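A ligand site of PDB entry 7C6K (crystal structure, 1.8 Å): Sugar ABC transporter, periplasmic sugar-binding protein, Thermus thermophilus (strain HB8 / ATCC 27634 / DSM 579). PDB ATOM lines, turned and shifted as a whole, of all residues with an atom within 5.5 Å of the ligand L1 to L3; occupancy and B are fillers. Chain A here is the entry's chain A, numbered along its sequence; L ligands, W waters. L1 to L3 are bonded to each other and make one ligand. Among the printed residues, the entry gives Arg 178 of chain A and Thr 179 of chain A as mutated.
The backbone NH of Gly 297 is in hydrogen-bond range of an oxygen (O1) of LG3 L3. O3 of LG2 L2 lies within hydrogen-bond range of NH2 of Arg 120 (3.4 Å). The backbone carbonyl oxygen (O) of Gly 297 lies close to an oxygen (O2) of LG3 L3 (3.3 Å). The side-chain hydroxyl of Thr 66 sits at hydrogen-bond distance from an oxygen (O2) of LG3 L3. The side-chain carboxylate (OE1) of Glu 118 lies within hydrogen-bond range of an oxygen (O1) of LG3 L3, at 2.5 Å. The guanidinium group (NH2) of Arg 260 sits at hydrogen-bond distance from an oxygen (O2) of LIG L1 (2.8 Å). The side-chain hydroxyl (OG1) of Thr 179 lies within hydrogen-bond range of an oxygen (O4) of LG4 L4 (2.9 Å). OG1 of Thr 236 sits at hydrogen-bond distance from O6 of LG4 L4 (2.5 Å). An oxygen (O3) of LG3 L3 is in hydrogen-bond range of the side-chain hydroxyl of Thr 67, at 2.6 Å. An oxygen (O7) of LG4 L4 lies within salt-bridge range of the guanidinium group of Arg 178. N of Thr 66 sits at hydrogen-bond distance from O3 of LG3 L3, 3.4 Å away. The backbone NH of Arg 178 is in hydrogen-bond range of an oxygen (O5) of LG4 L4, 3.0 Å away. An oxygen (O3) of LG3 L3 sits at hydrogen-bond distance from the backbone NH (N) of Thr 67, at 3.1 Å. The backbone carbonyl oxygen of Pro 11 sits at hydrogen-bond distance from an oxygen (O2) of LIG L1 (3.1 Å). N of Thr 179 lies within hydrogen-bond range of O5 of LG4 L4, at 3.0 Å. O1 of LG4 L4 lies within salt-bridge range of NH2 of Arg 120. The side-chain carboxylate (OE1) of Glu 240 is in hydrogen-bond range of an oxygen (O1) of LIG L1 (3.4 Å). A ring nitrogen (ND1) of His 181 is in hydrogen-bond range of an oxygen (O1) of LG4 L4 (2.6 Å).
NH2 of Arg 260 is in hydrogen-bond range of O of Asn 12 (3.0 Å). The backbone NH of Thr 66 is in hydrogen-bond range of the backbone carbonyl oxygen of Gly 297 (2.9 Å). O of Phe 116 sits at hydrogen-bond distance from N of Ser 298 (3.0 Å). The backbone NH of Arg 120 lies within hydrogen-bond range of the backbone carbonyl oxygen of Phe 294, 3.1 Å away. O of Glu 118 sits at hydrogen-bond distance from N of Gly 296 (2.7 Å). SD of Met 257 is in hydrogen-bond range of NE1 of Trp 256, at 3.8 Å. NE of Arg 120 is in salt-bridge range of OE2 of Glu 118 (2.8 Å). NE1 of Trp 256 is in hydrogen-bond range of OE2 of Glu 240, 3.3 Å away.
Water W1 lies within hydrogen-bond range of O5 of LG2 L2 (2.6 Å), OG of Ser 298 (2.7 Å) and O of Gly 297 (3.1 Å). Water W7 lies within hydrogen-bond range of an oxygen (O3) of LIG L1 (2.7 Å), the side-chain amide oxygen of Asn 12 (2.8 Å) and the indole nitrogen of Trp 42 (2.9 Å). Water W4 bridges an oxygen (O4) of LG4 L4 (2.7 Å) and an oxygen (O2) of LG2 L2 (2.8 Å). Water W5 bridges an oxygen (O1) of LG2 L2 (2.8 Å) and the guanidinium group of Arg 178 (3.3 Å). Water W2 bridges O5 of LG3 L3 (2.8 Å) and NE1 of Trp 68 (2.9 Å). Water W6 lies within hydrogen-bond range of OE1 of Glu 376 (2.7 Å), OG1 of Thr 67 (2.8 Å), NE2 of His 181 (2.9 Å) and O5 of LG3 L3 (3.2 Å).
Trp 42 touches the ligand L1 to L3. Gly 65 touches the ligand L1 to L3. NE1 of Trp 68 touches C5 of LG3 L3, 3.6 Å away. CE1 of Phe 116 touches O5 of LG2 L2 (3.9 Å). NH1 of Arg 178 touches O1 of LG2 L2 (3.7 Å). CG2 of Thr 179 touches O5 of LG3 L3 (3.4 Å). CE1 of His 181 touches O5 of LG3 L3, 3.4 Å away. Thr 236 touches the ligand L1 to L3. Trp 256 touches the ligand L1 to L3. CZ of Phe 294 touches O2 of LG3 L3 (3.7 Å). CA of Gly 296 touches O2 of LG3 L3 (3.4 Å). CE of Met 334 touches O3 of LIG L1, 3.8 Å away. Hydrophobic or aromatic side chains that line the ligand L1 to L3: Trp 42, Trp 68, Phe 116, His 181, Trp 256, Phe 294 and Met 334. Of the 28 residues printed, 20 come within 4 Å of the ligand L1 to L3.
O1 of LG2 L2 lies within hydrogen-bond range of O3 of LG4 L4, at 3.4 Å.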
ATOM      1  N   PRO A  11      16.380  -5.083  19.894  1.00  0.00           N
ATOM      2  CA  PRO A  11      16.071  -6.481  19.551  1.00  0.00           C
ATOM      3  C   PRO A  11      16.969  -7.490  20.291  1.00  0.00           C
ATOM      4  O   PRO A  11      17.905  -8.066  19.716  1.00  0.00           O
ATOM      5  CB  PRO A  11      16.258  -6.561  18.014  1.00  0.00           C
ATOM      6  CG  PRO A  11      16.447  -5.152  17.567  1.00  0.00           C
ATOM      7  CD  PRO A  11      16.933  -4.369  18.755  1.00  0.00           C
ATOM      8  N   ASN A  12      16.736  -7.682  21.578  1.00  0.00           N
ATOM      9  CA  ASN A  12      17.643  -8.462  22.481  1.00  0.00           C
ATOM     10  C   ASN A  12      17.339  -9.978  22.428  1.00  0.00           C
ATOM     11  O   ASN A  12      18.119 -10.756  22.972  1.00  0.00           O
ATOM     12  CB  ASN A  12      17.419  -8.003  23.936  1.00  0.00           C
ATOM     13  CG  ASN A  12      17.587  -6.493  24.082  1.00  0.00           C
ATOM     14  OD1 ASN A  12      18.539  -5.903  23.555  1.00  0.00           O
ATOM     15  ND2 ASN A  12      16.722  -5.854  24.841  1.00  0.00           N
ATOM     16  N   SER A  13      16.271 -10.417  21.768  1.00  0.00           N
ATOM     17  CA  SER A  13      15.890 -11.847  21.599  1.00  0.00           C
ATOM     18  C   SER A  13      15.106 -12.004  20.286  1.00  0.00           C
ATOM     19  O   SER A  13      14.786 -11.026  19.596  1.00  0.00           O
ATOM     20  CB  SER A  13      15.103 -12.258  22.820  1.00  0.00           C
ATOM     21  OG  SER A  13      13.889 -11.508  22.912  1.00  0.00           O
ATOM     22  N   TRP A  42      19.109  -1.557  16.515  1.00  0.00           N
ATOM     23  CA  TRP A  42      20.376  -0.990  17.013  1.00  0.00           C
ATOM     24  C   TRP A  42      20.908   0.110  16.049  1.00  0.00           C
ATOM     25  O   TRP A  42      21.509   1.045  16.526  1.00  0.00           O
ATOM     26  CB  TRP A  42      21.359  -2.159  17.199  1.00  0.00           C
ATOM     27  CG  TRP A  42      21.217  -2.797  18.547  1.00  0.00           C
ATOM     28  CD1 TRP A  42      20.824  -4.087  18.822  1.00  0.00           C
ATOM     29  CD2 TRP A  42      21.549  -2.206  19.821  1.00  0.00           C
ATOM     30  NE1 TRP A  42      20.813  -4.297  20.181  1.00  0.00           N
ATOM     31  CE2 TRP A  42      21.326  -3.196  20.814  1.00  0.00           C
ATOM     32  CE3 TRP A  42      22.058  -0.964  20.231  1.00  0.00           C
ATOM     33  CZ2 TRP A  42      21.481  -2.932  22.171  1.00  0.00           C
ATOM     34  CZ3 TRP A  42      22.211  -0.708  21.570  1.00  0.00           C
ATOM     35  CH2 TRP A  42      21.944  -1.686  22.518  1.00  0.00           C
ATOM     36  N   GLN A  63      15.672   1.528  26.947  1.00  0.00           N
ATOM     37  CA  GLN A  63      16.972   0.844  26.904  1.00  0.00           C
ATOM     38  C   GLN A  63      18.043   1.806  26.369  1.00  0.00           C
ATOM     39  O   GLN A  63      17.800   2.597  25.434  1.00  0.00           O
ATOM     40  CB  GLN A  63      16.824  -0.444  26.082  1.00  0.00           C
ATOM     41  CG  GLN A  63      18.078  -1.303  26.086  1.00  0.00           C
ATOM     42  CD  GLN A  63      17.884  -2.566  25.269  1.00  0.00           C
ATOM     43  OE1 GLN A  63      16.739  -2.975  24.976  1.00  0.00           O
ATOM     44  NE2 GLN A  63      18.964  -3.250  24.955  1.00  0.00           N
ATOM     45  N   GLY A  65      22.263   1.357  25.347  1.00  0.00           N
ATOM     46  CA  GLY A  65      23.569   0.729  25.477  1.00  0.00           C
ATOM     47  C   GLY A  65      24.392   1.379  26.565  1.00  0.00           C
ATOM     48  O   GLY A  65      24.406   2.620  26.700  1.00  0.00           O
ATOM     49  N   THR A  66      25.197   0.596  27.273  1.00  0.00           N
ATOM     50  CA  THR A  66      26.011   1.156  28.389  1.00  0.00           C
ATOM     51  C   THR A  66      26.849   2.343  27.892  1.00  0.00           C
ATOM     52  O   THR A  66      27.062   3.319  28.643  1.00  0.00           O
ATOM     53  CB  THR A  66      26.915   0.113  29.044  1.00  0.00           C
ATOM     54  OG1 THR A  66      27.625  -0.615  28.056  1.00  0.00           O
ATOM     55  CG2 THR A  66      26.170  -0.895  29.903  1.00  0.00           C
ATOM     56  N   THR A  67      27.303   2.312  26.633  1.00  0.00           N
ATOM     57  CA  THR A  67      28.293   3.257  26.125  1.00  0.00           C
ATOM     58  C   THR A  67      27.618   4.565  25.780  1.00  0.00           C
ATOM     59  O   THR A  67      28.331   5.517  25.440  1.00  0.00           O
ATOM     60  CB  THR A  67      29.110   2.721  24.923  1.00  0.00           C
ATOM     61  OG1 THR A  67      28.304   2.559  23.756  1.00  0.00           O
ATOM     62  CG2 THR A  67      29.835   1.469  25.348  1.00  0.00           C
ATOM     63  N   TRP A  68      26.300   4.608  25.792  1.00  0.00           N
ATOM     64  CA  TRP A  68      25.467   5.773  25.405  1.00  0.00           C
ATOM     65  C   TRP A  68      25.092   6.575  26.665  1.00  0.00           C
ATOM     66  O   TRP A  68      24.540   7.684  26.480  1.00  0.00           O
ATOM     67  CB  TRP A  68      24.195   5.392  24.665  1.00  0.00           C
ATOM     68  CG  TRP A  68      24.362   4.698  23.338  1.00  0.00           C
ATOM     69  CD1 TRP A  68      25.512   4.506  22.631  1.00  0.00           C
ATOM     70  CD2 TRP A  68      23.320   4.030  22.597  1.00  0.00           C
ATOM     71  NE1 TRP A  68      25.235   3.857  21.441  1.00  0.00           N
ATOM     72  CE2 TRP A  68      23.907   3.532  21.426  1.00  0.00           C
ATOM     73  CE3 TRP A  68      21.937   3.885  22.762  1.00  0.00           C
ATOM     74  CZ2 TRP A  68      23.172   2.872  20.431  1.00  0.00           C
ATOM     75  CZ3 TRP A  68      21.206   3.250  21.768  1.00  0.00           C
ATOM     76  CH2 TRP A  68      21.826   2.753  20.625  1.00  0.00           C
ATOM     77  N   PHE A 116      21.090  -5.670  31.651  1.00  0.00           N
ATOM     78  CA  PHE A 116      21.822  -6.898  31.376  1.00  0.00           C
ATOM     79  C   PHE A 116      23.255  -6.549  31.010  1.00  0.00           C
ATOM     80  O   PHE A 116      23.616  -5.390  30.619  1.00  0.00           O
ATOM     81  CB  PHE A 116      21.114  -7.763  30.324  1.00  0.00           C
ATOM     82  CG  PHE A 116      21.011  -7.200  28.926  1.00  0.00           C
ATOM     83  CD1 PHE A 116      22.075  -7.208  28.062  1.00  0.00           C
ATOM     84  CD2 PHE A 116      19.816  -6.642  28.487  1.00  0.00           C
ATOM     85  CE1 PHE A 116      21.953  -6.734  26.759  1.00  0.00           C
ATOM     86  CE2 PHE A 116      19.708  -6.142  27.203  1.00  0.00           C
ATOM     87  CZ  PHE A 116      20.778  -6.172  26.359  1.00  0.00           C
ATOM     88  N   GLU A 118      26.921  -8.059  28.829  1.00  0.00           N
ATOM     89  CA  GLU A 118      27.398  -8.974  27.781  1.00  0.00           C
ATOM     90  C   GLU A 118      28.869  -8.629  27.576  1.00  0.00           C
ATOM     91  O   GLU A 118      29.314  -7.546  27.930  1.00  0.00           O
ATOM     92  CB  GLU A 118      26.541  -8.871  26.506  1.00  0.00           C
ATOM     93  CG  GLU A 118      26.574  -7.533  25.779  1.00  0.00           C
ATOM     94  CD  GLU A 118      27.658  -7.327  24.713  1.00  0.00           C
ATOM     95  OE1 GLU A 118      27.775  -6.206  24.156  1.00  0.00           O
ATOM     96  OE2 GLU A 118      28.494  -8.289  24.499  1.00  0.00           O
ATOM     97  N   ARG A 120      32.598 -10.087  25.082  1.00  0.00           N
ATOM     98  CA  ARG A 120      32.925 -10.787  23.806  1.00  0.00           C
ATOM     99  C   ARG A 120      33.937 -11.904  24.033  1.00  0.00           C
ATOM    100  O   ARG A 120      34.837 -11.779  24.900  1.00  0.00           O
ATOM    101  CB  ARG A 120      33.386  -9.781  22.738  1.00  0.00           C
ATOM    102  CG  ARG A 120      32.446  -8.588  22.612  1.00  0.00           C
ATOM    103  CD  ARG A 120      31.051  -9.010  22.219  1.00  0.00           C
ATOM    104  NE  ARG A 120      30.043  -7.967  22.209  1.00  0.00           N
ATOM    105  CZ  ARG A 120      29.765  -7.069  21.265  1.00  0.00           C
ATOM    106  NH1 ARG A 120      30.433  -7.089  20.099  1.00  0.00           N
ATOM    107  NH2 ARG A 120      28.747  -6.221  21.481  1.00  0.00           N
ATOM    108  N   ARG A 178      30.274   0.126  13.093  1.00  0.00           N
ATOM    109  CA  ARG A 178      29.534   1.115  13.918  1.00  0.00           C
ATOM    110  C   ARG A 178      30.376   1.386  15.166  1.00  0.00           C
ATOM    111  O   ARG A 178      30.267   2.510  15.691  1.00  0.00           O
ATOM    112  CB  ARG A 178      28.179   0.612  14.462  1.00  0.00           C
ATOM    113  CG  ARG A 178      27.118   0.270  13.432  1.00  0.00           C
ATOM    114  CD  ARG A 178      26.008  -0.452  14.153  1.00  0.00           C
ATOM    115  NE  ARG A 178      24.998  -0.813  13.169  1.00  0.00           N
ATOM    116  CZ  ARG A 178      24.135  -1.793  13.351  1.00  0.00           C
ATOM    117  NH1 ARG A 178      24.199  -2.545  14.452  1.00  0.00           N
ATOM    118  NH2 ARG A 178      23.240  -2.018  12.406  1.00  0.00           N
ATOM    119  N   THR A 179      31.116   0.384  15.668  1.00  0.00           N
ATOM    120  CA  THR A 179      31.858   0.470  16.940  1.00  0.00           C
ATOM    121  C   THR A 179      33.263  -0.168  16.855  1.00  0.00           C
ATOM    122  O   THR A 179      33.608  -0.949  15.940  1.00  0.00           O
ATOM    123  CB  THR A 179      31.052  -0.124  18.098  1.00  0.00           C
ATOM    124  OG1 THR A 179      31.253  -1.523  17.997  1.00  0.00           O
ATOM    125  CG2 THR A 179      29.580   0.208  18.102  1.00  0.00           C
ATOM    126  N   HIS A 181      34.090  -2.339  19.147  1.00  0.00           N
ATOM    127  CA  HIS A 181      33.997  -3.558  19.983  1.00  0.00           C
ATOM    128  C   HIS A 181      34.940  -4.664  19.470  1.00  0.00           C
ATOM    129  O   HIS A 181      35.530  -5.326  20.313  1.00  0.00           O
ATOM    130  CB  HIS A 181      32.573  -4.090  20.089  1.00  0.00           C
ATOM    131  CG  HIS A 181      31.636  -3.052  20.641  1.00  0.00           C
ATOM    132  ND1 HIS A 181      30.257  -3.163  20.529  1.00  0.00           N
ATOM    133  CD2 HIS A 181      31.884  -1.852  21.206  1.00  0.00           C
ATOM    134  CE1 HIS A 181      29.716  -2.053  21.041  1.00  0.00           C
ATOM    135  NE2 HIS A 181      30.673  -1.245  21.458  1.00  0.00           N
ATOM    136  N   THR A 236      28.861  -6.728  10.608  1.00  0.00           N
ATOM    137  CA  THR A 236      28.827  -7.681  11.728  1.00  0.00           C
ATOM    138  C   THR A 236      27.696  -8.681  11.554  1.00  0.00           C
ATOM    139  O   THR A 236      27.897  -9.871  11.833  1.00  0.00           O
ATOM    140  CB  THR A 236      28.698  -6.979  13.081  1.00  0.00           C
ATOM    141  OG1 THR A 236      29.915  -6.263  13.301  1.00  0.00           O
ATOM    142  CG2 THR A 236      28.464  -7.972  14.185  1.00  0.00           C
ATOM    143  N   ALA A 237      26.507  -8.216  11.187  1.00  0.00           N
ATOM    144  CA  ALA A 237      25.342  -9.117  11.040  1.00  0.00           C
ATOM    145  C   ALA A 237      25.625 -10.152   9.966  1.00  0.00           C
ATOM    146  O   ALA A 237      25.169 -11.286  10.116  1.00  0.00           O
ATOM    147  CB  ALA A 237      24.134  -8.311  10.682  1.00  0.00           C
ATOM    148  N   GLU A 240      28.037 -12.799  11.233  1.00  0.00           N
ATOM    149  CA  GLU A 240      27.278 -13.683  12.172  1.00  0.00           C
ATOM    150  C   GLU A 240      26.465 -14.712  11.364  1.00  0.00           C
ATOM    151  O   GLU A 240      26.579 -15.897  11.596  1.00  0.00           O
ATOM    152  CB  GLU A 240      26.445 -12.831  13.098  1.00  0.00           C
ATOM    153  CG  GLU A 240      25.726 -13.662  14.152  1.00  0.00           C
ATOM    154  CD  GLU A 240      24.918 -12.827  15.138  1.00  0.00           C
ATOM    155  OE1 GLU A 240      23.672 -12.693  14.928  1.00  0.00           O
ATOM    156  OE2 GLU A 240      25.540 -12.299  16.102  1.00  0.00           O
ATOM    157  N   TRP A 256      24.853 -14.219  23.506  1.00  0.00           N
ATOM    158  CA  TRP A 256      23.487 -14.450  22.963  1.00  0.00           C
ATOM    159  C   TRP A 256      23.533 -15.588  21.959  1.00  0.00           C
ATOM    160  O   TRP A 256      22.507 -16.309  21.763  1.00  0.00           O
ATOM    161  CB  TRP A 256      22.894 -13.160  22.388  1.00  0.00           C
ATOM    162  CG  TRP A 256      23.662 -12.559  21.263  1.00  0.00           C
ATOM    163  CD1 TRP A 256      23.550 -12.811  19.919  1.00  0.00           C
ATOM    164  CD2 TRP A 256      24.624 -11.509  21.401  1.00  0.00           C
ATOM    165  NE1 TRP A 256      24.454 -12.056  19.228  1.00  0.00           N
ATOM    166  CE2 TRP A 256      25.128 -11.254  20.103  1.00  0.00           C
ATOM    167  CE3 TRP A 256      25.136 -10.789  22.482  1.00  0.00           C
ATOM    168  CZ2 TRP A 256      26.079 -10.262  19.841  1.00  0.00           C
ATOM    169  CZ3 TRP A 256      26.063  -9.797  22.211  1.00  0.00           C
ATOM    170  CH2 TRP A 256      26.538  -9.578  20.931  1.00  0.00           C
ATOM    171  N   MET A 257      24.656 -15.780  21.265  1.00  0.00           N
ATOM    172  CA  MET A 257      24.741 -16.779  20.186  1.00  0.00           C
ATOM    173  C   MET A 257      24.536 -18.187  20.776  1.00  0.00           C
ATOM    174  O   MET A 257      24.072 -19.076  20.036  1.00  0.00           O
ATOM    175  CB  MET A 257      26.080 -16.701  19.443  1.00  0.00           C
ATOM    176  CG  MET A 257      26.238 -15.436  18.635  1.00  0.00           C
ATOM    177  SD  MET A 257      24.947 -15.324  17.391  1.00  0.00           S
ATOM    178  CE  MET A 257      25.679 -16.479  16.255  1.00  0.00           C
ATOM    179  N   ARG A 260      20.818 -18.520  20.723  1.00  0.00           N
ATOM    180  CA  ARG A 260      20.332 -18.610  19.339  1.00  0.00           C
ATOM    181  C   ARG A 260      20.612 -20.022  18.798  1.00  0.00           C
ATOM    182  O   ARG A 260      19.838 -20.522  17.946  1.00  0.00           O
ATOM    183  CB  ARG A 260      20.920 -17.534  18.445  1.00  0.00           C
ATOM    184  CG  ARG A 260      20.690 -16.090  18.913  1.00  0.00           C
ATOM    185  CD  ARG A 260      19.203 -15.715  19.031  1.00  0.00           C
ATOM    186  NE  ARG A 260      19.205 -14.307  19.391  1.00  0.00           N
ATOM    187  CZ  ARG A 260      19.261 -13.844  20.652  1.00  0.00           C
ATOM    188  NH1 ARG A 260      19.263 -14.646  21.693  1.00  0.00           N
ATOM    189  NH2 ARG A 260      19.339 -12.563  20.861  1.00  0.00           N
ATOM    190  N   PHE A 294      36.035  -6.751  25.467  1.00  0.00           N
ATOM    191  CA  PHE A 294      35.009  -5.697  25.585  1.00  0.00           C
ATOM    192  C   PHE A 294      33.901  -6.242  26.493  1.00  0.00           C
ATOM    193  O   PHE A 294      33.354  -7.347  26.203  1.00  0.00           O
ATOM    194  CB  PHE A 294      34.483  -5.251  24.205  1.00  0.00           C
ATOM    195  CG  PHE A 294      33.317  -4.302  24.273  1.00  0.00           C
ATOM    196  CD1 PHE A 294      33.494  -2.974  24.595  1.00  0.00           C
ATOM    197  CD2 PHE A 294      32.029  -4.788  24.170  1.00  0.00           C
ATOM    198  CE1 PHE A 294      32.419  -2.131  24.764  1.00  0.00           C
ATOM    199  CE2 PHE A 294      30.936  -3.946  24.364  1.00  0.00           C
ATOM    200  CZ  PHE A 294      31.147  -2.625  24.618  1.00  0.00           C
ATOM    201  N   PHE A 295      33.509  -5.423  27.463  1.00  0.00           N
ATOM    202  CA  PHE A 295      32.420  -5.718  28.425  1.00  0.00           C
ATOM    203  C   PHE A 295      31.408  -4.627  28.231  1.00  0.00           C
ATOM    204  O   PHE A 295      31.746  -3.439  28.431  1.00  0.00           O
ATOM    205  CB  PHE A 295      32.968  -5.757  29.848  1.00  0.00           C
ATOM    206  CG  PHE A 295      32.012  -6.283  30.873  1.00  0.00           C
ATOM    207  CD1 PHE A 295      30.964  -5.497  31.326  1.00  0.00           C
ATOM    208  CD2 PHE A 295      32.088  -7.574  31.351  1.00  0.00           C
ATOM    209  CE1 PHE A 295      30.081  -5.991  32.286  1.00  0.00           C
ATOM    210  CE2 PHE A 295      31.216  -8.037  32.307  1.00  0.00           C
ATOM    211  CZ  PHE A 295      30.211  -7.239  32.773  1.00  0.00           C
ATOM    212  N   GLY A 296      30.196  -4.977  27.865  1.00  0.00           N
ATOM    213  CA  GLY A 296      29.127  -3.971  27.712  1.00  0.00           C
ATOM    214  C   GLY A 296      27.821  -4.467  28.292  1.00  0.00           C
ATOM    215  O   GLY A 296      27.819  -5.081  29.341  1.00  0.00           O
ATOM    216  N   GLY A 297      26.764  -4.225  27.591  1.00  0.00           N
ATOM    217  CA  GLY A 297      25.398  -4.446  28.016  1.00  0.00           C
ATOM    218  C   GLY A 297      24.538  -3.219  27.868  1.00  0.00           C
ATOM    219  O   GLY A 297      24.839  -2.316  27.101  1.00  0.00           O
ATOM    220  N   SER A 298      23.361  -3.287  28.459  1.00  0.00           N
ATOM    221  CA  SER A 298      22.318  -2.273  28.333  1.00  0.00           C
ATOM    222  C   SER A 298      21.741  -1.978  29.721  1.00  0.00           C
ATOM    223  O   SER A 298      21.692  -2.856  30.560  1.00  0.00           O
ATOM    224  CB  SER A 298      21.191  -2.682  27.393  1.00  0.00           C
ATOM    225  OG  SER A 298      21.624  -2.595  26.032  1.00  0.00           O
ATOM    226  N   MET A 334      21.724 -13.142  27.246  1.00  0.00           N
ATOM    227  CA  MET A 334      22.667 -12.196  27.856  1.00  0.00           C
ATOM    228  C   MET A 334      22.994 -12.665  29.278  1.00  0.00           C
ATOM    229  O   MET A 334      22.482 -13.674  29.720  1.00  0.00           O
ATOM    230  CB  MET A 334      22.085 -10.783  27.916  1.00  0.00           C
ATOM    231  CG  MET A 334      21.642 -10.263  26.572  1.00  0.00           C
ATOM    232  SD  MET A 334      22.936 -10.060  25.376  1.00  0.00           S
ATOM    233  CE  MET A 334      21.964  -9.534  23.954  1.00  0.00           C
ATOM    234  N   GLU A 376      34.041   7.618  19.305  1.00  0.00           N
ATOM    235  CA  GLU A 376      33.982   6.273  18.705  1.00  0.00           C
ATOM    236  C   GLU A 376      33.700   6.468  17.199  1.00  0.00           C
ATOM    237  O   GLU A 376      34.255   5.770  16.346  1.00  0.00           O
ATOM    238  CB  GLU A 376      32.909   5.440  19.404  1.00  0.00           C
ATOM    239  CG  GLU A 376      33.152   3.975  19.108  1.00  0.00           C
ATOM    240  CD  GLU A 376      32.520   2.957  19.992  1.00  0.00           C
ATOM    241  OE1 GLU A 376      31.541   3.279  20.680  1.00  0.00           O
ATOM    242  OE2 GLU A 376      33.021   1.823  19.964  1.00  0.00           O
HETATM  243  C1  LIG L   1      21.090 -10.225  18.617  1.00  0.00           C
HETATM  244  C2  LIG L   1      21.419  -8.765  18.899  1.00  0.00           C
HETATM  245  C3  LIG L   1      22.815  -8.445  18.363  1.00  0.00           C
HETATM  246  C4  LIG L   1      23.064  -8.871  16.901  1.00  0.00           C
HETATM  247  C5  LIG L   1      24.509  -8.778  16.490  1.00  0.00           C
HETATM  248  C6  LIG L   1      21.322 -10.523  17.136  1.00  0.00           C
HETATM  249  O1  LIG L   1      21.079 -11.885  17.022  1.00  0.00           O
HETATM  250  O2  LIG L   1      19.756 -10.519  19.059  1.00  0.00           O
HETATM  251  O3  LIG L   1      21.263  -8.539  20.305  1.00  0.00           O
HETATM  252  O4  LIG L   1      22.993  -7.048  18.305  1.00  0.00           O
HETATM  253  O5  LIG L   1      22.660 -10.230  16.727  1.00  0.00           O
HETATM  254  O6  LIG L   1      24.712  -8.696  15.078  1.00  0.00           O
HETATM  255  C1  LG2 L   2      24.166  -5.022  18.703  1.00  0.00           C
HETATM  256  C2  LG2 L   2      25.220  -4.399  19.592  1.00  0.00           C
HETATM  257  C3  LG2 L   2      24.893  -4.724  21.065  1.00  0.00           C
HETATM  258  C4  LG2 L   2      24.700  -6.214  21.296  1.00  0.00           C
HETATM  259  C5  LG2 L   2      24.295  -6.622  22.671  1.00  0.00           C
HETATM  260  C6  LG2 L   2      24.013  -6.492  19.063  1.00  0.00           C
HETATM  261  O1  LG2 L   2      24.524  -4.875  17.313  1.00  0.00           O
HETATM  262  O2  LG2 L   2      25.297  -3.006  19.339  1.00  0.00           O
HETATM  263  O3  LG2 L   2      25.971  -4.342  21.902  1.00  0.00           O
HETATM  264  O4  LG2 L   2      23.671  -6.692  20.430  1.00  0.00           O
HETATM  265  O5  LG2 L   2      23.148  -5.896  23.095  1.00  0.00           O
HETATM  266  C1  LG3 L   3      26.687  -3.123  23.819  1.00  0.00           C
HETATM  267  C2  LG3 L   3      26.648  -1.776  24.537  1.00  0.00           C
HETATM  268  C3  LG3 L   3      26.880  -0.629  23.564  1.00  0.00           C
HETATM  269  C4  LG3 L   3      25.935  -0.781  22.385  1.00  0.00           C
HETATM  270  C5  LG3 L   3      26.032   0.318  21.349  1.00  0.00           C
HETATM  271  C6  LG3 L   3      25.778  -3.131  22.597  1.00  0.00           C
HETATM  272  O1  LG3 L   3      26.369  -4.190  24.701  1.00  0.00           O
HETATM  273  O2  LG3 L   3      27.665  -1.796  25.552  1.00  0.00           O
HETATM  274  O3  LG3 L   3      26.592   0.621  24.186  1.00  0.00           O
HETATM  275  O4  LG3 L   3      26.128  -2.067  21.734  1.00  0.00           O
HETATM  276  O5  LG3 L   3      27.247   0.275  20.604  1.00  0.00           O
HETATM  277  P1  LG4 L   4      29.057  -4.700  17.653  1.00  0.00           P
HETATM  278  O1  LG4 L   4      28.724  -4.724  19.107  1.00  0.00           O
HETATM  279  O2  LG4 L   4      30.379  -5.417  17.447  1.00  0.00           O
HETATM  280  O3  LG4 L   4      27.839  -5.221  16.890  1.00  0.00           O
HETATM  281  O4  LG4 L   4      29.196  -3.221  16.963  1.00  0.00           O
HETATM  282  P2  LG4 L   4      29.419  -3.403  15.313  1.00  0.00           P
HETATM  283  O5  LG4 L   4      30.399  -2.394  14.778  1.00  0.00           O
HETATM  284  O6  LG4 L   4      30.114  -4.754  15.226  1.00  0.00           O
HETATM  285  O7  LG4 L   4      27.995  -3.460  14.691  1.00  0.00           O
HETATM  286  O   HOH W   1      23.556  -4.280  25.104  1.00  0.00           O
HETATM  287  O   HOH W   2      27.329   2.974  19.706  1.00  0.00           O
HETATM  288  O   HOH W   3      24.950  -6.158  13.762  1.00  0.00           O
HETATM  289  O   HOH W   4      26.739  -2.081  17.185  1.00  0.00           O
HETATM  290  O   HOH W   5      22.501  -5.167  15.413  1.00  0.00           O
HETATM  291  O   HOH W   6      29.923   1.488  21.791  1.00  0.00           O
HETATM  292  O   HOH W   7      20.709  -6.536  21.967  1.00  0.00           O
